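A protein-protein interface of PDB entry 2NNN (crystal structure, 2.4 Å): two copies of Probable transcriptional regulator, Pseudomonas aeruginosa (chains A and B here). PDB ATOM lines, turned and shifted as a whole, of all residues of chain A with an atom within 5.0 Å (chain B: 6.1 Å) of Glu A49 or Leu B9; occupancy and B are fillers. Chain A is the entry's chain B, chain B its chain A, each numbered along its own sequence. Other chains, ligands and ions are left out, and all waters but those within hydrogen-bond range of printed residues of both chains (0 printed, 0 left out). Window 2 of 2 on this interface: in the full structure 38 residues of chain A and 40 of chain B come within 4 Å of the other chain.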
ATOM      1  N   ALA A  42      -8.264  26.480   0.979  1.00  0.00           N
ATOM      2  CA  ALA A  42      -6.813  26.489   1.130  1.00  0.00           C
ATOM      3  C   ALA A  42      -6.351  27.750   1.841  1.00  0.00           C
ATOM      4  O   ALA A  42      -5.601  27.670   2.811  1.00  0.00           O
ATOM      5  CB  ALA A  42      -6.145  26.382  -0.236  1.00  0.00           C
ATOM      6  N   VAL A  45      -7.598  27.490   5.504  1.00  0.00           N
ATOM      7  CA  VAL A  45      -6.752  26.565   6.249  1.00  0.00           C
ATOM      8  C   VAL A  45      -5.401  27.201   6.567  1.00  0.00           C
ATOM      9  O   VAL A  45      -4.935  27.122   7.699  1.00  0.00           O
ATOM     10  CB  VAL A  45      -6.563  25.230   5.478  1.00  0.00           C
ATOM     11  CG1 VAL A  45      -5.534  24.320   6.159  1.00  0.00           C
ATOM     12  CG2 VAL A  45      -7.918  24.511   5.303  1.00  0.00           C
ATOM     13  N   ARG A  46      -4.789  27.839   5.576  1.00  0.00           N
ATOM     14  CA  ARG A  46      -3.473  28.430   5.755  1.00  0.00           C
ATOM     15  C   ARG A  46      -3.454  29.554   6.813  1.00  0.00           C
ATOM     16  O   ARG A  46      -2.554  29.590   7.645  1.00  0.00           O
ATOM     17  CB  ARG A  46      -2.882  28.886   4.420  1.00  0.00           C
ATOM     18  CG  ARG A  46      -1.394  29.232   4.481  1.00  0.00           C
ATOM     19  CD  ARG A  46      -0.542  28.005   4.759  1.00  0.00           C
ATOM     20  NE  ARG A  46      -0.182  27.331   3.517  1.00  0.00           N
ATOM     21  CZ  ARG A  46       0.373  26.123   3.432  1.00  0.00           C
ATOM     22  NH1 ARG A  46       0.639  25.409   4.524  1.00  0.00           N
ATOM     23  NH2 ARG A  46       0.655  25.623   2.242  1.00  0.00           N
ATOM     24  N   LEU A  47      -4.451  30.440   6.793  1.00  0.00           N
ATOM     25  CA  LEU A  47      -4.607  31.471   7.831  1.00  0.00           C
ATOM     26  C   LEU A  47      -4.822  30.914   9.243  1.00  0.00           C
ATOM     27  O   LEU A  47      -4.528  31.600  10.244  1.00  0.00           O
ATOM     28  CB  LEU A  47      -5.760  32.406   7.494  1.00  0.00           C
ATOM     29  CG  LEU A  47      -5.578  33.448   6.402  1.00  0.00           C
ATOM     30  CD1 LEU A  47      -6.898  34.155   6.195  1.00  0.00           C
ATOM     31  CD2 LEU A  47      -4.458  34.450   6.724  1.00  0.00           C
ATOM     32  N   GLY A  48      -5.363  29.694   9.323  1.00  0.00           N
ATOM     33  CA  GLY A  48      -5.439  28.955  10.573  1.00  0.00           C
ATOM     34  C   GLY A  48      -4.067  28.560  11.079  1.00  0.00           C
ATOM     35  O   GLY A  48      -3.818  28.595  12.279  1.00  0.00           O
ATOM     36  N   GLU A  49      -3.173  28.191  10.161  1.00  0.00           N
ATOM     37  CA  GLU A  49      -1.792  27.825  10.497  1.00  0.00           C
ATOM     38  C   GLU A  49      -0.910  29.026  10.861  1.00  0.00           C
ATOM     39  O   GLU A  49      -0.119  28.956  11.800  1.00  0.00           O
ATOM     40  CB  GLU A  49      -1.123  27.091   9.335  1.00  0.00           C
ATOM     41  CG  GLU A  49      -1.868  25.879   8.806  1.00  0.00           C
ATOM     42  CD  GLU A  49      -1.130  25.212   7.634  1.00  0.00           C
ATOM     43  OE1 GLU A  49       0.112  25.398   7.564  1.00  0.00           O
ATOM     44  OE2 GLU A  49      -1.786  24.508   6.804  1.00  0.00           O
ATOM     45  N   THR A  50      -1.045  30.115  10.107  1.00  0.00           N
ATOM     46  CA  THR A  50      -0.118  31.247  10.181  1.00  0.00           C
ATOM     47  C   THR A  50      -0.528  32.333  11.162  1.00  0.00           C
ATOM     48  O   THR A  50       0.311  33.057  11.682  1.00  0.00           O
ATOM     49  CB  THR A  50       0.026  31.935   8.810  1.00  0.00           C
ATOM     50  OG1 THR A  50      -1.265  32.357   8.360  1.00  0.00           O
ATOM     51  CG2 THR A  50       0.637  30.998   7.790  1.00  0.00           C
ATOM     52  N   GLY A  51      -1.824  32.459  11.400  1.00  0.00           N
ATOM     53  CA  GLY A  51      -2.337  33.614  12.109  1.00  0.00           C
ATOM     54  C   GLY A  51      -2.204  34.810  11.184  1.00  0.00           C
ATOM     55  O   GLY A  51      -2.136  34.639   9.963  1.00  0.00           O
ATOM     56  N   THR A  62       0.177  29.494  -0.639  1.00  0.00           N
ATOM     57  CA  THR A  62      -0.910  28.666  -1.175  1.00  0.00           C
ATOM     58  C   THR A  62      -0.907  28.655  -2.709  1.00  0.00           C
ATOM     59  O   THR A  62      -1.940  28.392  -3.315  1.00  0.00           O
ATOM     60  CB  THR A  62      -2.283  29.159  -0.709  1.00  0.00           C
ATOM     61  OG1 THR A  62      -2.430  30.533  -1.076  1.00  0.00           O
ATOM     62  CG2 THR A  62      -2.437  29.031   0.793  1.00  0.00           C
ATOM     63  N   TYR B   7      -4.203  17.785  10.160  1.00  0.00           N
ATOM     64  CA  TYR B   7      -4.662  18.418   8.878  1.00  0.00           C
ATOM     65  C   TYR B   7      -3.773  19.598   8.463  1.00  0.00           C
ATOM     66  O   TYR B   7      -4.010  20.750   8.857  1.00  0.00           O
ATOM     67  CB  TYR B   7      -6.146  18.850   8.959  1.00  0.00           C
ATOM     68  N   ARG B   8      -2.751  19.284   7.670  1.00  0.00           N
ATOM     69  CA  ARG B   8      -1.879  20.285   7.062  1.00  0.00           C
ATOM     70  C   ARG B   8      -2.209  20.371   5.572  1.00  0.00           C
ATOM     71  O   ARG B   8      -2.493  19.348   4.922  1.00  0.00           O
ATOM     72  CB  ARG B   8      -0.406  19.923   7.277  1.00  0.00           C
ATOM     73  N   LEU B   9      -2.168  21.590   5.039  1.00  0.00           N
ATOM     74  CA  LEU B   9      -2.574  21.840   3.659  1.00  0.00           C
ATOM     75  C   LEU B   9      -1.712  21.105   2.627  1.00  0.00           C
ATOM     76  O   LEU B   9      -2.247  20.571   1.644  1.00  0.00           O
ATOM     77  CB  LEU B   9      -2.630  23.353   3.374  1.00  0.00           C
ATOM     78  CG  LEU B   9      -3.123  23.874   2.015  1.00  0.00           C
ATOM     79  CD1 LEU B   9      -4.438  23.239   1.590  1.00  0.00           C
ATOM     80  CD2 LEU B   9      -3.243  25.395   2.063  1.00  0.00           C
ATOM     81  N   ASP B  10      -0.399  21.051   2.879  1.00  0.00           N
ATOM     82  CA  ASP B  10       0.585  20.516   1.915  1.00  0.00           C
ATOM     83  C   ASP B  10       0.550  18.998   1.734  1.00  0.00           C
ATOM     84  O   ASP B  10       1.214  18.458   0.853  1.00  0.00           O
ATOM     85  CB  ASP B  10       2.004  20.954   2.288  1.00  0.00           C
ATOM     86  CG  ASP B  10       2.106  22.443   2.543  1.00  0.00           C
ATOM     87  OD1 ASP B  10       2.462  23.190   1.599  1.00  0.00           O
ATOM     88  OD2 ASP B  10       1.805  22.861   3.685  1.00  0.00           O
ATOM     89  N   ASP B  11      -0.210  18.320   2.586  1.00  0.00           N
ATOM     90  CA  ASP B  11      -0.492  16.893   2.433  1.00  0.00           C
ATOM     91  C   ASP B  11      -1.767  16.645   1.630  1.00  0.00           C
ATOM     92  O   ASP B  11      -2.008  15.530   1.161  1.00  0.00           O
ATOM     93  CB  ASP B  11      -0.624  16.233   3.804  1.00  0.00           C
ATOM     94  CG  ASP B  11       0.649  16.337   4.614  1.00  0.00           C
ATOM     95  OD1 ASP B  11       1.752  16.219   4.025  1.00  0.00           O
ATOM     96  OD2 ASP B  11       0.544  16.543   5.843  1.00  0.00           O
ATOM     97  N   GLN B  12      -2.592  17.674   1.479  1.00  0.00           N
ATOM     98  CA  GLN B  12      -3.860  17.508   0.781  1.00  0.00           C
ATOM     99  C   GLN B  12      -3.578  17.329  -0.690  1.00  0.00           C
ATOM    100  O   GLN B  12      -2.923  18.163  -1.305  1.00  0.00           O
ATOM    101  CB  GLN B  12      -4.784  18.707   1.027  1.00  0.00           C
ATOM    102  CG  GLN B  12      -5.080  18.959   2.497  1.00  0.00           C
ATOM    103  CD  GLN B  12      -5.349  17.672   3.267  1.00  0.00           C
ATOM    104  OE1 GLN B  12      -6.302  16.936   2.968  1.00  0.00           O
ATOM    105  NE2 GLN B  12      -4.501  17.386   4.253  1.00  0.00           N
ATOM    106  N   ILE B  13      -4.062  16.225  -1.245  1.00  0.00           N
ATOM    107  CA  ILE B  13      -3.826  15.891  -2.641  1.00  0.00           C
ATOM    108  C   ILE B  13      -4.421  16.898  -3.627  1.00  0.00           C
ATOM    109  O   ILE B  13      -3.907  17.061  -4.725  1.00  0.00           O
ATOM    110  CB  ILE B  13      -4.245  14.436  -2.959  1.00  0.00           C
ATOM    111  CG1 ILE B  13      -3.624  13.960  -4.283  1.00  0.00           C
ATOM    112  CG2 ILE B  13      -5.765  14.289  -2.954  1.00  0.00           C
ATOM    113  CD1 ILE B  13      -2.138  13.673  -4.192  1.00  0.00           C
ATOM    114  N   PHE B  15      -4.447  20.305  -3.212  1.00  0.00           N
ATOM    115  CA  PHE B  15      -3.441  21.374  -3.251  1.00  0.00           C
ATOM    116  C   PHE B  15      -2.255  20.959  -4.133  1.00  0.00           C
ATOM    117  O   PHE B  15      -1.795  21.728  -4.980  1.00  0.00           O
ATOM    118  CB  PHE B  15      -2.989  21.676  -1.813  1.00  0.00           C
ATOM    119  CG  PHE B  15      -2.017  22.820  -1.686  1.00  0.00           C
ATOM    120  CD1 PHE B  15      -2.186  24.006  -2.418  1.00  0.00           C
ATOM    121  CD2 PHE B  15      -0.947  22.733  -0.797  1.00  0.00           C
ATOM    122  CE1 PHE B  15      -1.292  25.049  -2.300  1.00  0.00           C
ATOM    123  CE2 PHE B  15      -0.042  23.790  -0.667  1.00  0.00           C
ATOM    124  CZ  PHE B  15      -0.220  24.950  -1.413  1.00  0.00           C
ATOM    125  N   ILE B  16      -1.791  19.725  -3.937  1.00  0.00           N
ATOM    126  CA  ILE B  16      -0.695  19.143  -4.705  1.00  0.00           C
ATOM    127  C   ILE B  16      -1.052  19.062  -6.193  1.00  0.00           C
ATOM    128  O   ILE B  16      -0.286  19.497  -7.032  1.00  0.00           O
ATOM    129  CB  ILE B  16      -0.326  17.738  -4.145  1.00  0.00           C
ATOM    130  CG1 ILE B  16       0.098  17.846  -2.661  1.00  0.00           C
ATOM    131  CG2 ILE B  16       0.759  17.064  -5.001  1.00  0.00           C
ATOM    132  CD1 ILE B  16       0.477  16.514  -2.013  1.00  0.00           C
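Of the printed residues of chain B, Ala A42 touches Leu B9 (3.4 Å). Of the printed residues of chain B, Arg A46 touches Leu B9, Asp B10 and Phe B15. Leu A47 touches none of the printed residues of chain B. Of the printed residues of chain B, Thr A62 touches Leu B9 and Phe B15. Tyr B7 touches none of the printed residues of chain A. Of chain A, only Ala A42, Arg A46, Glu A49 and Thr A62 come within 4 Å of Leu B9. Of the printed residues of chain A, Asp B10 touches Arg A46. Of the printed residues of chain A, Phe B15 touches Arg A46 and Thr A62.
No position is printed for both chains.
N of Leu B9 lies within hydrogen-bond range of OE2 of Glu A49 (3.4 Å). The side-chain carboxylate (OD2) of Asp B10 lies within salt-bridge range of the guanidinium group (NH1) of Arg A46, at 2.9 Å.
O of Ala A42 touches CD2 of Leu B9, at 3.4 Å. Leu B9 touches Arg A46 (CD2 to NE, 3.9 Å). Phe B15 touches Arg A46 (CE2 to NH2, 3.5 Å). Thr A62 touches Leu B9 (CG2 to CD2, 3.9 Å). Thr A62 touches Phe B15.
OE1 of Glu A49 lies within salt-bridge range of NH1 of Arg A46, 3.1 Å away. OG1 of Thr A50 lies within hydrogen-bond range of O of Arg A46, at 3.1 Å.
Printed residues of chain A that touch a printed residue of chain B: Ala A42, Arg A46, Glu A49 and Thr A62. Hydrophobic or aromatic side chains of chain A within 4 Å of the printed part of chain B: Ala A42. Printed residues of chain B that touch a printed residue of chain A: Leu B9, Asp B10 and Phe B15. Among the printed residues, 7 pairs touch across the chains. Among the printed residues, Asp or Glu carboxylates within 4 Å of a Lys or Arg side-chain nitrogen of the other chain: Arg A46 with Asp B10.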
